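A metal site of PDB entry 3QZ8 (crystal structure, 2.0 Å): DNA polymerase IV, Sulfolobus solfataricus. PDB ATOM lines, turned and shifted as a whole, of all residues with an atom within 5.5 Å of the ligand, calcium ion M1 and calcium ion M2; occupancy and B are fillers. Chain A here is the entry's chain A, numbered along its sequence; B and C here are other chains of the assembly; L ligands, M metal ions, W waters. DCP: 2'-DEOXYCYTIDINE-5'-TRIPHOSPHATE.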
ATOM      1  N   ASP A   7      18.374  16.966   8.893  1.00  0.00           N
ATOM      2  CA  ASP A   7      18.737  18.379   8.776  1.00  0.00           C
ATOM      3  C   ASP A   7      19.667  18.640   9.939  1.00  0.00           C
ATOM      4  O   ASP A   7      19.278  18.452  11.072  1.00  0.00           O
ATOM      5  CB  ASP A   7      17.461  19.234   8.898  1.00  0.00           C
ATOM      6  CG  ASP A   7      17.699  20.740   8.726  1.00  0.00           C
ATOM      7  OD1 ASP A   7      18.828  21.216   8.883  1.00  0.00           O
ATOM      8  OD2 ASP A   7      16.708  21.452   8.424  1.00  0.00           O
ATOM      9  N   PHE A   8      20.922  18.996   9.667  1.00  0.00           N
ATOM     10  CA  PHE A   8      21.934  19.084  10.734  1.00  0.00           C
ATOM     11  C   PHE A   8      21.687  20.373  11.553  1.00  0.00           C
ATOM     12  O   PHE A   8      21.293  21.391  10.973  1.00  0.00           O
ATOM     13  CB  PHE A   8      23.362  19.106  10.170  1.00  0.00           C
ATOM     14  CG  PHE A   8      23.654  18.048   9.125  1.00  0.00           C
ATOM     15  CD1 PHE A   8      22.883  16.902   9.024  1.00  0.00           C
ATOM     16  CD2 PHE A   8      24.738  18.199   8.285  1.00  0.00           C
ATOM     17  CE1 PHE A   8      23.181  15.925   8.060  1.00  0.00           C
ATOM     18  CE2 PHE A   8      25.045  17.229   7.311  1.00  0.00           C
ATOM     19  CZ  PHE A   8      24.250  16.094   7.197  1.00  0.00           C
ATOM     20  N   ASP A   9      21.892  20.325  12.866  1.00  0.00           N
ATOM     21  CA  ASP A   9      21.533  21.461  13.738  1.00  0.00           C
ATOM     22  C   ASP A   9      22.563  22.599  13.691  1.00  0.00           C
ATOM     23  O   ASP A   9      23.755  22.338  13.735  1.00  0.00           O
ATOM     24  CB  ASP A   9      21.392  21.005  15.205  1.00  0.00           C
ATOM     25  CG  ASP A   9      20.237  20.022  15.436  1.00  0.00           C
ATOM     26  OD1 ASP A   9      19.205  20.107  14.737  1.00  0.00           O
ATOM     27  OD2 ASP A   9      20.372  19.159  16.337  1.00  0.00           O
ATOM     28  N   TYR A  10      22.111  23.847  13.669  1.00  0.00           N
ATOM     29  CA  TYR A  10      23.015  25.003  13.621  1.00  0.00           C
ATOM     30  C   TYR A  10      24.379  24.661  12.999  1.00  0.00           C
ATOM     31  O   TYR A  10      25.442  24.919  13.548  1.00  0.00           O
ATOM     32  CB  TYR A  10      23.151  25.660  15.008  1.00  0.00           C
ATOM     33  CG  TYR A  10      23.684  24.816  16.142  1.00  0.00           C
ATOM     34  CD1 TYR A  10      24.951  25.073  16.696  1.00  0.00           C
ATOM     35  CD2 TYR A  10      22.935  23.788  16.697  1.00  0.00           C
ATOM     36  CE1 TYR A  10      25.453  24.308  17.774  1.00  0.00           C
ATOM     37  CE2 TYR A  10      23.431  23.003  17.767  1.00  0.00           C
ATOM     38  CZ  TYR A  10      24.687  23.286  18.298  1.00  0.00           C
ATOM     39  OH  TYR A  10      25.192  22.539  19.338  1.00  0.00           O
ATOM     40  N   PHE A  11      24.317  24.127  11.786  1.00  0.00           N
ATOM     41  CA  PHE A  11      25.427  23.359  11.271  1.00  0.00           C
ATOM     42  C   PHE A  11      26.787  24.036  11.331  1.00  0.00           C
ATOM     43  O   PHE A  11      27.697  23.464  11.906  1.00  0.00           O
ATOM     44  CB  PHE A  11      25.154  22.837   9.846  1.00  0.00           C
ATOM     45  CG  PHE A  11      26.207  21.897   9.356  1.00  0.00           C
ATOM     46  CD1 PHE A  11      26.609  20.812  10.137  1.00  0.00           C
ATOM     47  CD2 PHE A  11      26.821  22.087   8.124  1.00  0.00           C
ATOM     48  CE1 PHE A  11      27.609  19.924   9.678  1.00  0.00           C
ATOM     49  CE2 PHE A  11      27.813  21.203   7.660  1.00  0.00           C
ATOM     50  CZ  PHE A  11      28.219  20.127   8.441  1.00  0.00           C
ATOM     51  N   TYR A  12      26.966  25.225  10.745  1.00  0.00           N
ATOM     52  CA  TYR A  12      28.324  25.761  10.710  1.00  0.00           C
ATOM     53  C   TYR A  12      28.800  25.991  12.144  1.00  0.00           C
ATOM     54  O   TYR A  12      29.946  25.674  12.476  1.00  0.00           O
ATOM     55  CB  TYR A  12      28.437  27.082   9.948  1.00  0.00           C
ATOM     56  CG  TYR A  12      28.211  27.013   8.437  1.00  0.00           C
ATOM     57  CD1 TYR A  12      27.905  25.805   7.806  1.00  0.00           C
ATOM     58  CD2 TYR A  12      28.303  28.164   7.659  1.00  0.00           C
ATOM     59  CE1 TYR A  12      27.660  25.755   6.437  1.00  0.00           C
ATOM     60  CE2 TYR A  12      28.066  28.131   6.267  1.00  0.00           C
ATOM     61  CZ  TYR A  12      27.748  26.909   5.668  1.00  0.00           C
ATOM     62  OH  TYR A  12      27.523  26.828   4.306  1.00  0.00           O
ATOM     63  N   ALA A  13      27.959  26.559  12.992  1.00  0.00           N
ATOM     64  CA  ALA A  13      28.403  26.834  14.366  1.00  0.00           C
ATOM     65  C   ALA A  13      28.717  25.555  15.122  1.00  0.00           C
ATOM     66  O   ALA A  13      29.670  25.483  15.909  1.00  0.00           O
ATOM     67  CB  ALA A  13      27.388  27.628  15.114  1.00  0.00           C
ATOM     68  N   VAL A  43      25.830  37.611   9.022  1.00  0.00           N
ATOM     69  CA  VAL A  43      25.870  36.356   9.760  1.00  0.00           C
ATOM     70  C   VAL A  43      25.445  35.177   8.872  1.00  0.00           C
ATOM     71  O   VAL A  43      24.398  35.240   8.228  1.00  0.00           O
ATOM     72  CB  VAL A  43      24.949  36.422  10.985  1.00  0.00           C
ATOM     73  CG1 VAL A  43      24.863  35.057  11.659  1.00  0.00           C
ATOM     74  CG2 VAL A  43      25.448  37.479  11.950  1.00  0.00           C
ATOM     75  N   ALA A  44      26.243  34.099   8.853  1.00  0.00           N
ATOM     76  CA  ALA A  44      25.897  32.883   8.129  1.00  0.00           C
ATOM     77  C   ALA A  44      24.970  32.023   8.977  1.00  0.00           C
ATOM     78  O   ALA A  44      23.940  31.552   8.502  1.00  0.00           O
ATOM     79  CB  ALA A  44      27.138  32.114   7.734  1.00  0.00           C
ATOM     80  N   THR A  45      25.352  31.791  10.213  1.00  0.00           N
ATOM     81  CA  THR A  45      24.434  31.195  11.179  1.00  0.00           C
ATOM     82  C   THR A  45      24.958  31.488  12.581  1.00  0.00           C
ATOM     83  O   THR A  45      26.063  31.986  12.733  1.00  0.00           O
ATOM     84  CB  THR A  45      24.298  29.679  11.016  1.00  0.00           C
ATOM     85  OG1 THR A  45      23.117  29.250  11.706  1.00  0.00           O
ATOM     86  CG2 THR A  45      25.513  28.956  11.624  1.00  0.00           C
ATOM     87  N   ALA A  46      24.143  31.203  13.602  1.00  0.00           N
ATOM     88  CA  ALA A  46      24.533  31.361  14.999  1.00  0.00           C
ATOM     89  C   ALA A  46      23.988  30.168  15.761  1.00  0.00           C
ATOM     90  O   ALA A  46      22.968  29.595  15.341  1.00  0.00           O
ATOM     91  CB  ALA A  46      23.936  32.638  15.568  1.00  0.00           C
ATOM     92  N   TYR A  48      22.314  28.183  19.110  1.00  0.00           N
ATOM     93  CA  TYR A  48      21.054  28.553  19.744  1.00  0.00           C
ATOM     94  C   TYR A  48      21.279  29.518  20.912  1.00  0.00           C
ATOM     95  O   TYR A  48      20.400  30.291  21.252  1.00  0.00           O
ATOM     96  CB  TYR A  48      20.272  27.294  20.138  1.00  0.00           C
ATOM     97  CG  TYR A  48      19.552  26.656  18.943  1.00  0.00           C
ATOM     98  CD1 TYR A  48      18.193  26.897  18.714  1.00  0.00           C
ATOM     99  CD2 TYR A  48      20.236  25.847  18.021  1.00  0.00           C
ATOM    100  CE1 TYR A  48      17.529  26.329  17.634  1.00  0.00           C
ATOM    101  CE2 TYR A  48      19.580  25.275  16.946  1.00  0.00           C
ATOM    102  CZ  TYR A  48      18.226  25.516  16.752  1.00  0.00           C
ATOM    103  OH  TYR A  48      17.539  24.961  15.681  1.00  0.00           O
ATOM    104  N   ARG A  51      21.215  32.724  18.978  1.00  0.00           N
ATOM    105  CA  ARG A  51      20.002  32.929  18.216  1.00  0.00           C
ATOM    106  C   ARG A  51      18.856  33.308  19.128  1.00  0.00           C
ATOM    107  O   ARG A  51      17.952  34.037  18.745  1.00  0.00           O
ATOM    108  CB  ARG A  51      19.671  31.635  17.465  1.00  0.00           C
ATOM    109  CG  ARG A  51      18.746  31.810  16.304  1.00  0.00           C
ATOM    110  CD  ARG A  51      18.457  30.469  15.661  1.00  0.00           C
ATOM    111  NE  ARG A  51      19.654  29.875  15.065  1.00  0.00           N
ATOM    112  CZ  ARG A  51      19.636  28.773  14.331  1.00  0.00           C
ATOM    113  NH1 ARG A  51      18.492  28.151  14.076  1.00  0.00           N
ATOM    114  NH2 ARG A  51      20.768  28.297  13.821  1.00  0.00           N
ATOM    115  N   ALA A  57      20.778  34.216  11.007  1.00  0.00           N
ATOM    116  CA  ALA A  57      21.308  34.192   9.656  1.00  0.00           C
ATOM    117  C   ALA A  57      20.810  35.384   8.894  1.00  0.00           C
ATOM    118  O   ALA A  57      19.620  35.706   8.923  1.00  0.00           O
ATOM    119  CB  ALA A  57      20.885  32.914   8.952  1.00  0.00           C
ATOM    120  N   GLY A  58      21.726  36.071   8.214  1.00  0.00           N
ATOM    121  CA  GLY A  58      21.352  37.133   7.316  1.00  0.00           C
ATOM    122  C   GLY A  58      21.562  38.520   7.892  1.00  0.00           C
ATOM    123  O   GLY A  58      21.833  39.449   7.160  1.00  0.00           O
ATOM    124  N   MET A  76      33.603  32.328   8.548  1.00  0.00           N
ATOM    125  CA  MET A  76      33.088  31.103   7.926  1.00  0.00           C
ATOM    126  C   MET A  76      34.258  30.297   7.312  1.00  0.00           C
ATOM    127  O   MET A  76      35.098  30.854   6.637  1.00  0.00           O
ATOM    128  CB  MET A  76      32.041  31.493   6.855  1.00  0.00           C
ATOM    129  CG  MET A  76      31.430  30.319   6.135  1.00  0.00           C
ATOM    130  SD  MET A  76      30.260  30.825   4.893  1.00  0.00           S
ATOM    131  CE  MET A  76      31.337  31.544   3.643  1.00  0.00           C
ATOM    132  N   SER A 103      21.226  19.903   0.266  1.00  0.00           N
ATOM    133  CA  SER A 103      22.081  21.063   0.520  1.00  0.00           C
ATOM    134  C   SER A 103      23.210  20.582   1.381  1.00  0.00           C
ATOM    135  O   SER A 103      23.334  19.394   1.633  1.00  0.00           O
ATOM    136  CB  SER A 103      21.339  22.178   1.243  1.00  0.00           C
ATOM    137  OG  SER A 103      21.116  21.799   2.586  1.00  0.00           O
ATOM    138  N   ILE A 104      24.004  21.500   1.880  1.00  0.00           N
ATOM    139  CA  ILE A 104      25.189  21.083   2.624  1.00  0.00           C
ATOM    140  C   ILE A 104      24.803  20.391   3.934  1.00  0.00           C
ATOM    141  O   ILE A 104      25.602  19.650   4.501  1.00  0.00           O
ATOM    142  CB  ILE A 104      26.089  22.292   2.927  1.00  0.00           C
ATOM    143  CG1 ILE A 104      27.403  21.835   3.556  1.00  0.00           C
ATOM    144  CG2 ILE A 104      25.343  23.255   3.847  1.00  0.00           C
ATOM    145  CD1 ILE A 104      28.504  22.828   3.411  1.00  0.00           C
ATOM    146  N   ASP A 105      23.599  20.634   4.447  1.00  0.00           N
ATOM    147  CA  ASP A 105      23.247  20.000   5.721  1.00  0.00           C
ATOM    148  C   ASP A 105      21.869  19.317   5.756  1.00  0.00           C
ATOM    149  O   ASP A 105      21.299  19.159   6.819  1.00  0.00           O
ATOM    150  CB  ASP A 105      23.357  21.030   6.837  1.00  0.00           C
ATOM    151  CG  ASP A 105      22.094  21.858   6.983  1.00  0.00           C
ATOM    152  OD1 ASP A 105      21.498  22.168   5.939  1.00  0.00           O
ATOM    153  OD2 ASP A 105      21.700  22.156   8.133  1.00  0.00           O
ATOM    154  N   GLU A 106      21.376  18.860   4.614  1.00  0.00           N
ATOM    155  CA  GLU A 106      20.067  18.214   4.555  1.00  0.00           C
ATOM    156  C   GLU A 106      20.079  17.087   3.561  1.00  0.00           C
ATOM    157  O   GLU A 106      20.688  17.203   2.503  1.00  0.00           O
ATOM    158  CB  GLU A 106      19.005  19.168   4.022  1.00  0.00           C
ATOM    159  CG  GLU A 106      18.880  20.443   4.738  1.00  0.00           C
ATOM    160  CD  GLU A 106      17.936  21.356   3.997  1.00  0.00           C
ATOM    161  OE1 GLU A 106      18.268  21.729   2.855  1.00  0.00           O
ATOM    162  OE2 GLU A 106      16.857  21.649   4.524  1.00  0.00           O
ATOM    163  N   LYS A 159      12.986  20.634  15.543  1.00  0.00           N
ATOM    164  CA  LYS A 159      14.269  21.295  15.755  1.00  0.00           C
ATOM    165  C   LYS A 159      14.293  21.929  17.148  1.00  0.00           C
ATOM    166  O   LYS A 159      13.302  22.517  17.561  1.00  0.00           O
ATOM    167  CB  LYS A 159      14.472  22.391  14.703  1.00  0.00           C
ATOM    168  CG  LYS A 159      15.308  21.969  13.533  1.00  0.00           C
ATOM    169  CD  LYS A 159      15.326  23.067  12.461  1.00  0.00           C
ATOM    170  CE  LYS A 159      15.886  22.547  11.128  1.00  0.00           C
ATOM    171  NZ  LYS A 159      16.282  23.629  10.136  1.00  0.00           N
ATOM    172  N   PRO A 160      15.431  21.846  17.834  1.00  0.00           N
ATOM    173  CA  PRO A 160      16.668  21.178  17.420  1.00  0.00           C
ATOM    174  C   PRO A 160      16.856  19.832  18.077  1.00  0.00           C
ATOM    175  O   PRO A 160      16.151  19.508  19.020  1.00  0.00           O
ATOM    176  CB  PRO A 160      17.735  22.119  17.957  1.00  0.00           C
ATOM    177  CG  PRO A 160      17.156  22.533  19.256  1.00  0.00           C
ATOM    178  CD  PRO A 160      15.666  22.672  19.024  1.00  0.00           C
ATOM    179  P    DG B   5      27.892  43.427   2.865  1.00  0.00           P
ATOM    180  OP1  DG B   5      29.054  44.349   2.776  1.00  0.00           O
ATOM    181  OP2  DG B   5      26.892  43.285   1.774  1.00  0.00           O
ATOM    182  O5'  DG B   5      28.520  41.986   3.147  1.00  0.00           O
ATOM    183  C5'  DG B   5      27.686  40.850   3.196  1.00  0.00           C
ATOM    184  C4'  DG B   5      28.555  39.670   2.888  1.00  0.00           C
ATOM    185  O4'  DG B   5      27.888  38.470   3.347  1.00  0.00           O
ATOM    186  C3'  DG B   5      28.780  39.452   1.390  1.00  0.00           C
ATOM    187  O3'  DG B   5      30.000  38.715   1.268  1.00  0.00           O
ATOM    188  C2'  DG B   5      27.507  38.696   1.031  1.00  0.00           C
ATOM    189  C1'  DG B   5      27.328  37.780   2.243  1.00  0.00           C
ATOM    190  N9   DG B   5      25.982  37.439   2.696  1.00  0.00           N
ATOM    191  C8   DG B   5      24.893  38.255   2.804  1.00  0.00           C
ATOM    192  N7   DG B   5      23.853  37.626   3.285  1.00  0.00           N
ATOM    193  C5   DG B   5      24.261  36.316   3.519  1.00  0.00           C
ATOM    194  C6   DG B   5      23.571  35.188   4.036  1.00  0.00           C
ATOM    195  O6   DG B   5      22.394  35.092   4.411  1.00  0.00           O
ATOM    196  N1   DG B   5      24.386  34.052   4.096  1.00  0.00           N
ATOM    197  C2   DG B   5      25.708  34.029   3.714  1.00  0.00           C
ATOM    198  N2   DG B   5      26.356  32.848   3.841  1.00  0.00           N
ATOM    199  N3   DG B   5      26.372  35.084   3.250  1.00  0.00           N
ATOM    200  C4   DG B   5      25.584  36.194   3.164  1.00  0.00           C
ATOM    201  P    DC B   6      30.689  38.503  -0.177  1.00  0.00           P
ATOM    202  OP1  DC B   6      32.126  38.299   0.029  1.00  0.00           O
ATOM    203  OP2  DC B   6      30.139  39.506  -1.096  1.00  0.00           O
ATOM    204  O5'  DC B   6      30.089  37.117  -0.666  1.00  0.00           O
ATOM    205  C5'  DC B   6      30.489  36.009   0.099  1.00  0.00           C
ATOM    206  C4'  DC B   6      29.668  34.818  -0.334  1.00  0.00           C
ATOM    207  O4'  DC B   6      28.353  34.853   0.249  1.00  0.00           O
ATOM    208  C3'  DC B   6      29.522  34.661  -1.866  1.00  0.00           C
ATOM    209  O3'  DC B   6      30.252  33.479  -1.939  1.00  0.00           O
ATOM    210  C2'  DC B   6      28.005  34.569  -2.065  1.00  0.00           C
ATOM    211  C1'  DC B   6      27.488  34.219  -0.671  1.00  0.00           C
ATOM    212  N1   DC B   6      26.095  34.600  -0.329  1.00  0.00           N
ATOM    213  C2   DC B   6      25.350  33.608   0.273  1.00  0.00           C
ATOM    214  O2   DC B   6      25.910  32.520   0.461  1.00  0.00           O
ATOM    215  N3   DC B   6      24.074  33.853   0.645  1.00  0.00           N
ATOM    216  C4   DC B   6      23.555  35.051   0.409  1.00  0.00           C
ATOM    217  N4   DC B   6      22.284  35.227   0.781  1.00  0.00           N
ATOM    218  C5   DC B   6      24.294  36.090  -0.209  1.00  0.00           C
ATOM    219  C6   DC B   6      25.561  35.829  -0.557  1.00  0.00           C
ATOM    220  P    DG C  13      15.749  26.081   4.086  1.00  0.00           P
ATOM    221  OP1  DG C  13      15.078  24.852   4.572  1.00  0.00           O
ATOM    222  OP2  DG C  13      15.600  27.338   4.853  1.00  0.00           O
ATOM    223  O5'  DG C  13      17.312  25.806   3.905  1.00  0.00           O
ATOM    224  C5'  DG C  13      17.785  24.990   2.822  1.00  0.00           C
ATOM    225  C4'  DG C  13      19.298  25.160   2.685  1.00  0.00           C
ATOM    226  O4'  DG C  13      19.530  26.427   1.998  1.00  0.00           O
ATOM    227  C3'  DG C  13      20.121  25.215   3.986  1.00  0.00           C
ATOM    228  O3'  DG C  13      21.371  24.539   3.836  1.00  0.00           O
ATOM    229  C2'  DG C  13      20.387  26.700   4.155  1.00  0.00           C
ATOM    230  C1'  DG C  13      20.502  27.157   2.689  1.00  0.00           C
ATOM    231  N9   DG C  13      20.235  28.595   2.555  1.00  0.00           N
ATOM    232  C8   DG C  13      19.094  29.285   2.878  1.00  0.00           C
ATOM    233  N7   DG C  13      19.212  30.566   2.643  1.00  0.00           N
ATOM    234  C5   DG C  13      20.516  30.726   2.179  1.00  0.00           C
ATOM    235  C6   DG C  13      21.240  31.879   1.780  1.00  0.00           C
ATOM    236  O6   DG C  13      20.879  33.069   1.744  1.00  0.00           O
ATOM    237  N1   DG C  13      22.531  31.566   1.366  1.00  0.00           N
ATOM    238  C2   DG C  13      23.080  30.313   1.363  1.00  0.00           C
ATOM    239  N2   DG C  13      24.349  30.225   0.955  1.00  0.00           N
ATOM    240  N3   DG C  13      22.419  29.225   1.724  1.00  0.00           N
ATOM    241  C4   DG C  13      21.155  29.511   2.112  1.00  0.00           C
HETATM  242  N1  DCP L   1      23.401  29.301   5.783  1.00  0.00           N
HETATM  243  C2  DCP L   1      23.943  30.524   5.235  1.00  0.00           C
HETATM  244  N3  DCP L   1      23.115  31.666   5.022  1.00  0.00           N
HETATM  245  C4  DCP L   1      21.726  31.617   5.353  1.00  0.00           C
HETATM  246  C5  DCP L   1      21.140  30.396   5.917  1.00  0.00           C
HETATM  247  C6  DCP L   1      22.025  29.237   6.146  1.00  0.00           C
HETATM  248  O2  DCP L   1      25.118  30.603   4.919  1.00  0.00           O
HETATM  249  N4  DCP L   1      20.935  32.784   5.116  1.00  0.00           N
HETATM  250  C1' DCP L   1      24.292  28.163   6.020  1.00  0.00           C
HETATM  251  C2' DCP L   1      24.759  28.126   7.424  1.00  0.00           C
HETATM  252  C3' DCP L   1      23.850  27.176   8.093  1.00  0.00           C
HETATM  253  C4' DCP L   1      23.544  26.196   7.063  1.00  0.00           C
HETATM  254  O4' DCP L   1      23.673  26.943   5.800  1.00  0.00           O
HETATM  255  O3' DCP L   1      24.489  26.602   9.194  1.00  0.00           O
HETATM  256  C5' DCP L   1      22.193  25.501   7.268  1.00  0.00           C
HETATM  257  O5' DCP L   1      20.982  26.236   7.282  1.00  0.00           O
HETATM  258  PA  DCP L   1      19.805  26.048   8.352  1.00  0.00           P
HETATM  259  O1A DCP L   1      19.070  26.983   7.377  1.00  0.00           O
HETATM  260  O2A DCP L   1      19.783  24.539   8.144  1.00  0.00           O
HETATM  261  O3A DCP L   1      20.684  26.631   9.571  1.00  0.00           O
HETATM  262  PB  DCP L   1      21.305  25.901  10.866  1.00  0.00           P
HETATM  263  O1B DCP L   1      21.531  24.536  10.227  1.00  0.00           O
HETATM  264  O2B DCP L   1      22.377  27.030  10.827  1.00  0.00           O
HETATM  265  O3B DCP L   1      20.050  26.164  11.743  1.00  0.00           O
HETATM  266  PG  DCP L   1      19.004  25.087  12.191  1.00  0.00           P
HETATM  267  O1G DCP L   1      18.790  24.131  11.058  1.00  0.00           O
HETATM  268  O2G DCP L   1      17.759  25.932  12.385  1.00  0.00           O
HETATM  269  O3G DCP L   1      19.392  24.312  13.426  1.00  0.00           O
HETATM  270 CA    CA M   1      20.195  22.854   9.668  1.00  0.00          CA
HETATM  271 CA    CA M   2      19.118  22.992   6.448  1.00  0.00          CA
HETATM  272  O   HOH W   1      24.002  26.449   2.570  1.00  0.00           O
HETATM  273  O   HOH W   2      26.960  29.227   3.200  1.00  0.00           O
HETATM  274  O   HOH W   3      16.676  23.356   6.402  1.00  0.00           O
HETATM  275  O   HOH W   4      18.351  32.941   5.818  1.00  0.00           O
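Calcium ion M1 is bound by an oxygen (O1B) of the ligand (2.2 Å), the backbone carbonyl oxygen (O) of Phe 8 (2.2 Å), the side-chain carboxylate (OD2) of Asp 105 (2.3 Å), the side-chain carboxylate (OD1) of Asp 7 (2.3 Å), an oxygen (O2A) of the ligand (2.3 Å) and an oxygen (O1G) of the ligand (2.4 Å).
Three residues have an atom within 4 Å of calcium ion M1: Asp 7, Phe 8 and Asp 105.
Residues that only touch the ligand: Ala 44, Asp 9 and Ala 57.
Hydrophobic or aromatic side chains that line the ligand: Phe 11, Tyr 12, Ala 44, Tyr 48 and Ala 57.
Within 4 Å of the ligand: Asp 7, Phe 8, Asp 9, Tyr 10, Phe 11, Tyr 12, Ala 44, Thr 45, Tyr 48, Arg 51, Ala 57, Asp 105, Lys 159, DG 5 of chain B and DG 13 of chain C.
Calcium ion M2 is bound by an oxygen (O2A) of the ligand (2.4 Å), water W3 (2.5 Å) and the side-chain carboxylate of Asp 105 (2.6 Å).
Slightly farther from calcium ion M2 lies the side-chain carboxylate (OD1) of Asp 7 (3.0 Å).
CG of Glu 106 touches calcium ion M2, 3.1 Å away.
C3' of DG 13 of chain C touches calcium ion M2, at 3.5 Å.
Four residues have an atom within 4 Å of calcium ion M2: Asp 7, Asp 105, Glu 106 and DG 13 of chain C.
Water W2 bridges the side-chain hydroxyl (OH) of Tyr 12 (2.7 Å) and an oxygen (O2) of the ligand (2.9 Å).
Water W1 bridges O4' of the ligand (3.3 Å) and N3 of DG 13 of chain C (3.3 Å).
The side-chain hydroxyl (OG1) of Thr 45 is in hydrogen-bond range of an oxygen (O2B) of the ligand (2.5 Å).
The side-chain amino group (NZ) of Lys 159 lies within salt-bridge range of an oxygen (O2G) of the ligand.
N of Tyr 10 sits at hydrogen-bond distance from O3G of the ligand, 2.8 Å away.
N4 of the ligand is in hydrogen-bond range of O6 of DG 5 of chain B (2.8 Å).
The guanidinium group (NH1) of Arg 51 lies within salt-bridge range of an oxygen (O2G) of the ligand (2.9 Å).
O3G of the ligand sits at hydrogen-bond distance from OH of Tyr 48, 3.0 Å away.
N4 of the ligand sits at hydrogen-bond distance from O6 of DG 13 of chain C, at 3.4 Å.
N of Phe 11 lies close to O1B of the ligand.
An oxygen (O3') of the ligand lies within hydrogen-bond range of the backbone NH of Tyr 12 (3.2 Å).
N of Asp 105 lies close to OG of Ser 103, at 3.3 Å.
NZ of Lys 159 lies within salt-bridge range of OD2 of Asp 7 (2.8 Å).
OG1 of Thr 45 lies within hydrogen-bond range of NH2 of Arg 51.
The backbone carbonyl oxygen of Ala 46 lies within hydrogen-bond range of the guanidinium group of Arg 51 (3.0 Å).
The side-chain hydroxyl (OG) of Ser 103 lies within hydrogen-bond range of the side-chain carboxylate (OE1) of Glu 106 (2.9 Å).
O3' of DG 13 of chain C lies within hydrogen-bond range of the side-chain hydroxyl of Ser 103, at 3.0 Å.
O6 of DG 13 of chain C sits close to N4 of DC 6 of chain B, 2.7 Å away.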
